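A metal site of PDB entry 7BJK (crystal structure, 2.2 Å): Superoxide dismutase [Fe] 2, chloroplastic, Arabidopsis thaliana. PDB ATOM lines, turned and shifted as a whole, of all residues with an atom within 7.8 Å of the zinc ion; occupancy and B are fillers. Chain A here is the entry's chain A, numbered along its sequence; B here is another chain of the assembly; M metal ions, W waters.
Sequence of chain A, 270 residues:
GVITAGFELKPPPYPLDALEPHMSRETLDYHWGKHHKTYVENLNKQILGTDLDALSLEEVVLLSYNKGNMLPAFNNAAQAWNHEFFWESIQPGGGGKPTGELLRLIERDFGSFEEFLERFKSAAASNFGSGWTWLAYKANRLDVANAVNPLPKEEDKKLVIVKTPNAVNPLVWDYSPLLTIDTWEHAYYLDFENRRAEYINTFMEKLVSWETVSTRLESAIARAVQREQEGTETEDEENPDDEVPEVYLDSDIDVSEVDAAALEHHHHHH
O of His 31 lies within hydrogen-bond range of N of His 36, at 3.0 Å.
O of Gln 79 lies within hydrogen-bond range of ND1 of His 83 (2.7 Å).
The backbone carbonyl oxygen (O) of His 83 sits close to the indole nitrogen (NE1) of Trp 87 (3.3 Å).
O of Asp 182 is in hydrogen-bond range of OH of Tyr 199, at 2.7 Å.
N of Trp 184 is in hydrogen-bond range of OD1 of Asp 182 (3.1 Å).
A ring nitrogen (ND1) of His 186 sits at hydrogen-bond distance from the side-chain carboxylate (OE2) of Glu 185 of chain B, at 2.7 Å.
Four residues have an atom within 4 Å of the zinc ion: His 31, His 83, Asp 182 and His 186.
Water W1 lies within hydrogen-bond range of OD1 of Asp 182 (2.9 Å) and NE2 of Gln 79 (3.2 Å).
The zinc ion is bound by OD2 of Asp 182 (1.9 Å), NE2 of His 186 (2.0 Å), NE2 of His 83 (2.0 Å), NE2 of His 31 (2.1 Å) and water W1 (2.2 Å).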
ATOM      1  N   HIS A  31     -19.550  35.568  21.457  1.00  0.00           N
ATOM      2  CA  HIS A  31     -19.128  34.536  20.512  1.00  0.00           C
ATOM      3  C   HIS A  31     -17.609  34.477  20.400  1.00  0.00           C
ATOM      4  O   HIS A  31     -16.995  33.415  20.527  1.00  0.00           O
ATOM      5  CB  HIS A  31     -19.772  34.784  19.149  1.00  0.00           C
ATOM      6  CG  HIS A  31     -19.718  33.604  18.240  1.00  0.00           C
ATOM      7  ND1 HIS A  31     -20.210  33.635  16.946  1.00  0.00           N
ATOM      8  CD2 HIS A  31     -19.261  32.341  18.428  1.00  0.00           C
ATOM      9  CE1 HIS A  31     -20.051  32.452  16.385  1.00  0.00           C
ATOM     10  NE2 HIS A  31     -19.479  31.650  17.266  1.00  0.00           N
ATOM     11  N   TRP A  32     -16.974  35.618  20.141  1.00  0.00           N
ATOM     12  CA  TRP A  32     -15.516  35.638  20.121  1.00  0.00           C
ATOM     13  C   TRP A  32     -14.937  35.687  21.535  1.00  0.00           C
ATOM     14  O   TRP A  32     -14.106  34.849  21.888  1.00  0.00           O
ATOM     15  CB  TRP A  32     -15.016  36.825  19.291  1.00  0.00           C
ATOM     16  CG  TRP A  32     -13.556  36.997  19.327  1.00  0.00           C
ATOM     17  CD1 TRP A  32     -12.646  36.325  18.568  1.00  0.00           C
ATOM     18  CD2 TRP A  32     -12.820  37.904  20.140  1.00  0.00           C
ATOM     19  NE1 TRP A  32     -11.386  36.751  18.863  1.00  0.00           N
ATOM     20  CE2 TRP A  32     -11.453  37.724  19.826  1.00  0.00           C
ATOM     21  CE3 TRP A  32     -13.176  38.854  21.101  1.00  0.00           C
ATOM     22  CZ2 TRP A  32     -10.435  38.449  20.451  1.00  0.00           C
ATOM     23  CZ3 TRP A  32     -12.158  39.580  21.726  1.00  0.00           C
ATOM     24  CH2 TRP A  32     -10.809  39.374  21.394  1.00  0.00           C
ATOM     25  N   HIS A  35     -16.721  32.024  23.593  1.00  0.00           N
ATOM     26  CA  HIS A  35     -16.685  30.688  22.993  1.00  0.00           C
ATOM     27  C   HIS A  35     -15.379  30.453  22.262  1.00  0.00           C
ATOM     28  O   HIS A  35     -14.709  29.433  22.478  1.00  0.00           O
ATOM     29  CB  HIS A  35     -17.864  30.493  22.042  1.00  0.00           C
ATOM     30  CG  HIS A  35     -19.083  29.941  22.707  1.00  0.00           C
ATOM     31  ND1 HIS A  35     -19.148  28.643  23.172  1.00  0.00           N
ATOM     32  CD2 HIS A  35     -20.281  30.504  22.997  1.00  0.00           C
ATOM     33  CE1 HIS A  35     -20.333  28.432  23.713  1.00  0.00           C
ATOM     34  NE2 HIS A  35     -21.038  29.542  23.631  1.00  0.00           N
ATOM     35  N   HIS A  36     -15.023  31.366  21.347  1.00  0.00           N
ATOM     36  CA  HIS A  36     -13.795  31.197  20.573  1.00  0.00           C
ATOM     37  C   HIS A  36     -12.583  31.180  21.508  1.00  0.00           C
ATOM     38  O   HIS A  36     -11.767  30.252  21.437  1.00  0.00           O
ATOM     39  CB  HIS A  36     -13.686  32.306  19.531  1.00  0.00           C
ATOM     40  CG  HIS A  36     -12.562  32.101  18.543  1.00  0.00           C
ATOM     41  ND1 HIS A  36     -12.331  32.958  17.495  1.00  0.00           N
ATOM     42  CD2 HIS A  36     -11.613  31.135  18.455  1.00  0.00           C
ATOM     43  CE1 HIS A  36     -11.296  32.533  16.789  1.00  0.00           C
ATOM     44  NE2 HIS A  36     -10.839  31.435  17.367  1.00  0.00           N
ATOM     45  N   TYR A  39     -12.414  27.765  23.159  1.00  0.00           N
ATOM     46  CA  TYR A  39     -11.879  26.718  22.292  1.00  0.00           C
ATOM     47  C   TYR A  39     -10.354  26.775  22.270  1.00  0.00           C
ATOM     48  O   TYR A  39      -9.682  25.756  22.429  1.00  0.00           O
ATOM     49  CB  TYR A  39     -12.435  26.843  20.866  1.00  0.00           C
ATOM     50  CG  TYR A  39     -13.915  26.490  20.730  1.00  0.00           C
ATOM     51  CD1 TYR A  39     -14.416  25.270  21.164  1.00  0.00           C
ATOM     52  CD2 TYR A  39     -14.812  27.389  20.171  1.00  0.00           C
ATOM     53  CE1 TYR A  39     -15.743  24.954  21.027  1.00  0.00           C
ATOM     54  CE2 TYR A  39     -16.161  27.082  20.040  1.00  0.00           C
ATOM     55  CZ  TYR A  39     -16.627  25.865  20.468  1.00  0.00           C
ATOM     56  OH  TYR A  39     -17.984  25.568  20.342  1.00  0.00           O
ATOM     57  N   GLN A  79     -12.678  23.725  16.042  1.00  0.00           N
ATOM     58  CA  GLN A  79     -13.479  24.898  16.355  1.00  0.00           C
ATOM     59  C   GLN A  79     -12.629  26.156  16.352  1.00  0.00           C
ATOM     60  O   GLN A  79     -13.082  27.196  15.856  1.00  0.00           O
ATOM     61  CB  GLN A  79     -14.176  24.739  17.697  1.00  0.00           C
ATOM     62  CG  GLN A  79     -15.392  23.825  17.630  1.00  0.00           C
ATOM     63  CD  GLN A  79     -16.465  24.358  16.692  1.00  0.00           C
ATOM     64  OE1 GLN A  79     -16.341  24.288  15.476  1.00  0.00           O
ATOM     65  NE2 GLN A  79     -17.532  24.898  17.257  1.00  0.00           N
ATOM     66  N   ASN A  82     -12.208  26.844  12.667  1.00  0.00           N
ATOM     67  CA  ASN A  82     -13.483  27.268  12.088  1.00  0.00           C
ATOM     68  C   ASN A  82     -13.832  28.706  12.465  1.00  0.00           C
ATOM     69  O   ASN A  82     -14.266  29.488  11.615  1.00  0.00           O
ATOM     70  CB  ASN A  82     -14.607  26.330  12.502  1.00  0.00           C
ATOM     71  CG  ASN A  82     -14.372  24.908  12.046  1.00  0.00           C
ATOM     72  OD1 ASN A  82     -13.582  24.669  11.143  1.00  0.00           O
ATOM     73  ND2 ASN A  82     -15.052  23.955  12.689  1.00  0.00           N
ATOM     74  N   HIS A  83     -13.614  29.076  13.727  1.00  0.00           N
ATOM     75  CA  HIS A  83     -14.044  30.403  14.168  1.00  0.00           C
ATOM     76  C   HIS A  83     -13.176  31.499  13.590  1.00  0.00           C
ATOM     77  O   HIS A  83     -13.684  32.565  13.222  1.00  0.00           O
ATOM     78  CB  HIS A  83     -14.102  30.458  15.690  1.00  0.00           C
ATOM     79  CG  HIS A  83     -15.327  29.799  16.263  1.00  0.00           C
ATOM     80  ND1 HIS A  83     -15.419  28.426  16.409  1.00  0.00           N
ATOM     81  CD2 HIS A  83     -16.522  30.309  16.663  1.00  0.00           C
ATOM     82  CE1 HIS A  83     -16.606  28.127  16.907  1.00  0.00           C
ATOM     83  NE2 HIS A  83     -17.290  29.247  17.068  1.00  0.00           N
ATOM     84  N   PHE A  86     -14.404  31.914  10.256  1.00  0.00           N
ATOM     85  CA  PHE A  86     -15.691  32.605  10.330  1.00  0.00           C
ATOM     86  C   PHE A  86     -15.537  34.131  10.392  1.00  0.00           C
ATOM     87  O   PHE A  86     -16.173  34.852   9.622  1.00  0.00           O
ATOM     88  CB  PHE A  86     -16.479  32.097  11.529  1.00  0.00           C
ATOM     89  CG  PHE A  86     -17.873  32.660  11.639  1.00  0.00           C
ATOM     90  CD1 PHE A  86     -18.829  32.394  10.666  1.00  0.00           C
ATOM     91  CD2 PHE A  86     -18.242  33.455  12.724  1.00  0.00           C
ATOM     92  CE1 PHE A  86     -20.124  32.905  10.767  1.00  0.00           C
ATOM     93  CE2 PHE A  86     -19.523  33.970  12.840  1.00  0.00           C
ATOM     94  CZ  PHE A  86     -20.478  33.693  11.854  1.00  0.00           C
ATOM     95  N   TRP A  87     -14.715  34.640  11.329  1.00  0.00           N
ATOM     96  CA  TRP A  87     -14.641  36.098  11.470  1.00  0.00           C
ATOM     97  C   TRP A  87     -14.087  36.742  10.204  1.00  0.00           C
ATOM     98  O   TRP A  87     -14.421  37.886   9.889  1.00  0.00           O
ATOM     99  CB  TRP A  87     -13.781  36.532  12.671  1.00  0.00           C
ATOM    100  CG  TRP A  87     -14.205  35.881  13.929  1.00  0.00           C
ATOM    101  CD1 TRP A  87     -13.457  35.053  14.720  1.00  0.00           C
ATOM    102  CD2 TRP A  87     -15.515  35.938  14.516  1.00  0.00           C
ATOM    103  NE1 TRP A  87     -14.215  34.617  15.773  1.00  0.00           N
ATOM    104  CE2 TRP A  87     -15.483  35.129  15.668  1.00  0.00           C
ATOM    105  CE3 TRP A  87     -16.702  36.596  14.184  1.00  0.00           C
ATOM    106  CZ2 TRP A  87     -16.595  34.962  16.492  1.00  0.00           C
ATOM    107  CZ3 TRP A  87     -17.815  36.439  15.006  1.00  0.00           C
ATOM    108  CH2 TRP A  87     -17.747  35.622  16.153  1.00  0.00           C
ATOM    109  N   GLY A 131     -23.545  23.098  14.051  1.00  0.00           N
ATOM    110  CA  GLY A 131     -22.621  22.853  12.953  1.00  0.00           C
ATOM    111  C   GLY A 131     -22.391  24.059  12.052  1.00  0.00           C
ATOM    112  O   GLY A 131     -22.621  25.205  12.436  1.00  0.00           O
ATOM    113  N   TRP A 132     -21.954  23.739  10.831  1.00  0.00           N
ATOM    114  CA  TRP A 132     -21.431  24.704   9.872  1.00  0.00           C
ATOM    115  C   TRP A 132     -21.883  24.346   8.476  1.00  0.00           C
ATOM    116  O   TRP A 132     -22.012  23.155   8.133  1.00  0.00           O
ATOM    117  CB  TRP A 132     -19.896  24.726   9.876  1.00  0.00           C
ATOM    118  CG  TRP A 132     -19.300  24.958  11.212  1.00  0.00           C
ATOM    119  CD1 TRP A 132     -19.094  24.030  12.204  1.00  0.00           C
ATOM    120  CD2 TRP A 132     -18.797  26.200  11.735  1.00  0.00           C
ATOM    121  NE1 TRP A 132     -18.492  24.621  13.298  1.00  0.00           N
ATOM    122  CE2 TRP A 132     -18.308  25.955  13.033  1.00  0.00           C
ATOM    123  CE3 TRP A 132     -18.709  27.501  11.206  1.00  0.00           C
ATOM    124  CZ2 TRP A 132     -17.754  26.950  13.825  1.00  0.00           C
ATOM    125  CZ3 TRP A 132     -18.132  28.488  11.993  1.00  0.00           C
ATOM    126  CH2 TRP A 132     -17.669  28.220  13.294  1.00  0.00           C
ATOM    127  N   ASP A 182     -21.436  29.898  10.737  1.00  0.00           N
ATOM    128  CA  ASP A 182     -21.597  29.186  12.001  1.00  0.00           C
ATOM    129  C   ASP A 182     -23.087  29.077  12.313  1.00  0.00           C
ATOM    130  O   ASP A 182     -23.753  30.112  12.438  1.00  0.00           O
ATOM    131  CB  ASP A 182     -20.873  29.945  13.103  1.00  0.00           C
ATOM    132  CG  ASP A 182     -20.735  29.172  14.411  1.00  0.00           C
ATOM    133  OD1 ASP A 182     -21.307  28.066  14.588  1.00  0.00           O
ATOM    134  OD2 ASP A 182     -20.028  29.701  15.297  1.00  0.00           O
ATOM    135  N   THR A 183     -23.624  27.863  12.429  1.00  0.00           N
ATOM    136  CA  THR A 183     -25.043  27.739  12.789  1.00  0.00           C
ATOM    137  C   THR A 183     -25.214  27.039  14.131  1.00  0.00           C
ATOM    138  O   THR A 183     -26.330  26.588  14.461  1.00  0.00           O
ATOM    139  CB  THR A 183     -25.869  27.061  11.692  1.00  0.00           C
ATOM    140  OG1 THR A 183     -25.345  25.761  11.352  1.00  0.00           O
ATOM    141  CG2 THR A 183     -25.936  27.953  10.440  1.00  0.00           C
ATOM    142  N   TRP A 184     -24.146  26.940  14.915  1.00  0.00           N
ATOM    143  CA  TRP A 184     -24.288  26.758  16.356  1.00  0.00           C
ATOM    144  C   TRP A 184     -25.212  27.837  16.936  1.00  0.00           C
ATOM    145  O   TRP A 184     -25.133  29.007  16.549  1.00  0.00           O
ATOM    146  CB  TRP A 184     -22.905  26.851  17.031  1.00  0.00           C
ATOM    147  CG  TRP A 184     -22.067  25.629  16.892  1.00  0.00           C
ATOM    148  CD1 TRP A 184     -21.598  25.087  15.728  1.00  0.00           C
ATOM    149  CD2 TRP A 184     -21.597  24.802  17.943  1.00  0.00           C
ATOM    150  NE1 TRP A 184     -20.859  23.953  16.009  1.00  0.00           N
ATOM    151  CE2 TRP A 184     -20.848  23.764  17.364  1.00  0.00           C
ATOM    152  CE3 TRP A 184     -21.733  24.827  19.338  1.00  0.00           C
ATOM    153  CZ2 TRP A 184     -20.250  22.761  18.119  1.00  0.00           C
ATOM    154  CZ3 TRP A 184     -21.129  23.834  20.084  1.00  0.00           C
ATOM    155  CH2 TRP A 184     -20.397  22.820  19.472  1.00  0.00           C
ATOM    156  N   GLU A 185     -26.079  27.450  17.869  1.00  0.00           N
ATOM    157  CA  GLU A 185     -27.039  28.416  18.401  1.00  0.00           C
ATOM    158  C   GLU A 185     -26.342  29.639  18.984  1.00  0.00           C
ATOM    159  O   GLU A 185     -26.849  30.765  18.866  1.00  0.00           O
ATOM    160  CB  GLU A 185     -27.949  27.767  19.444  1.00  0.00           C
ATOM    161  CG  GLU A 185     -28.802  26.593  18.896  1.00  0.00           C
ATOM    162  CD  GLU A 185     -29.725  25.986  19.955  1.00  0.00           C
ATOM    163  OE1 GLU A 185     -29.201  25.607  21.032  1.00  0.00           O
ATOM    164  OE2 GLU A 185     -30.960  25.877  19.704  1.00  0.00           O
ATOM    165  N   HIS A 186     -25.160  29.452  19.587  1.00  0.00           N
ATOM    166  CA  HIS A 186     -24.496  30.586  20.212  1.00  0.00           C
ATOM    167  C   HIS A 186     -24.169  31.650  19.186  1.00  0.00           C
ATOM    168  O   HIS A 186     -23.951  32.804  19.552  1.00  0.00           O
ATOM    169  CB  HIS A 186     -23.237  30.137  20.966  1.00  0.00           C
ATOM    170  CG  HIS A 186     -22.130  29.622  20.091  1.00  0.00           C
ATOM    171  ND1 HIS A 186     -21.549  28.396  20.293  1.00  0.00           N
ATOM    172  CD2 HIS A 186     -21.480  30.191  19.048  1.00  0.00           C
ATOM    173  CE1 HIS A 186     -20.587  28.218  19.394  1.00  0.00           C
ATOM    174  NE2 HIS A 186     -20.532  29.294  18.634  1.00  0.00           N
ATOM    175  N   ALA A 187     -24.145  31.284  17.904  1.00  0.00           N
ATOM    176  CA  ALA A 187     -23.748  32.235  16.885  1.00  0.00           C
ATOM    177  C   ALA A 187     -24.822  33.257  16.586  1.00  0.00           C
ATOM    178  O   ALA A 187     -24.497  34.305  16.028  1.00  0.00           O
ATOM    179  CB  ALA A 187     -23.334  31.524  15.595  1.00  0.00           C
ATOM    180  N   TYR A 188     -26.095  32.985  16.932  1.00  0.00           N
ATOM    181  CA  TYR A 188     -27.143  33.927  16.562  1.00  0.00           C
ATOM    182  C   TYR A 188     -28.229  34.158  17.618  1.00  0.00           C
ATOM    183  O   TYR A 188     -29.136  34.961  17.361  1.00  0.00           O
ATOM    184  CB  TYR A 188     -27.796  33.509  15.245  1.00  0.00           C
ATOM    185  CG  TYR A 188     -28.394  32.116  15.244  1.00  0.00           C
ATOM    186  CD1 TYR A 188     -27.615  31.005  14.949  1.00  0.00           C
ATOM    187  CD2 TYR A 188     -29.743  31.903  15.506  1.00  0.00           C
ATOM    188  CE1 TYR A 188     -28.156  29.728  14.932  1.00  0.00           C
ATOM    189  CE2 TYR A 188     -30.283  30.624  15.475  1.00  0.00           C
ATOM    190  CZ  TYR A 188     -29.479  29.538  15.192  1.00  0.00           C
ATOM    191  OH  TYR A 188     -29.997  28.255  15.184  1.00  0.00           O
ATOM    192  N   TYR A 199     -31.152  34.915  10.585  1.00  0.00           N
ATOM    193  CA  TYR A 199     -29.704  34.981  10.729  1.00  0.00           C
ATOM    194  C   TYR A 199     -29.006  34.646   9.422  1.00  0.00           C
ATOM    195  O   TYR A 199     -28.173  35.416   8.936  1.00  0.00           O
ATOM    196  CB  TYR A 199     -29.283  34.024  11.835  1.00  0.00           C
ATOM    197  CG  TYR A 199     -27.829  33.706  11.868  1.00  0.00           C
ATOM    198  CD1 TYR A 199     -26.876  34.707  12.032  1.00  0.00           C
ATOM    199  CD2 TYR A 199     -27.396  32.396  11.783  1.00  0.00           C
ATOM    200  CE1 TYR A 199     -25.553  34.407  12.085  1.00  0.00           C
ATOM    201  CE2 TYR A 199     -26.079  32.086  11.844  1.00  0.00           C
ATOM    202  CZ  TYR A 199     -25.154  33.094  12.006  1.00  0.00           C
ATOM    203  OH  TYR A 199     -23.813  32.757  12.066  1.00  0.00           O
ATOM    204  N   GLU B 185     -27.361  24.267  23.562  1.00  0.00           N
ATOM    205  CA  GLU B 185     -26.964  25.563  24.114  1.00  0.00           C
ATOM    206  C   GLU B 185     -28.160  26.377  24.573  1.00  0.00           C
ATOM    207  O   GLU B 185     -28.054  27.154  25.524  1.00  0.00           O
ATOM    208  CB  GLU B 185     -26.125  26.339  23.090  1.00  0.00           C
ATOM    209  CG  GLU B 185     -24.705  25.802  22.934  1.00  0.00           C
ATOM    210  CD  GLU B 185     -23.845  26.572  21.919  1.00  0.00           C
ATOM    211  OE1 GLU B 185     -24.340  26.887  20.803  1.00  0.00           O
ATOM    212  OE2 GLU B 185     -22.668  26.851  22.248  1.00  0.00           O
HETATM  213 ZN    ZN M   1     -19.313  29.554  17.041  1.00  0.00          ZN
HETATM  214  O   HOH W   1     -19.449  27.391  16.685  1.00  0.00           O
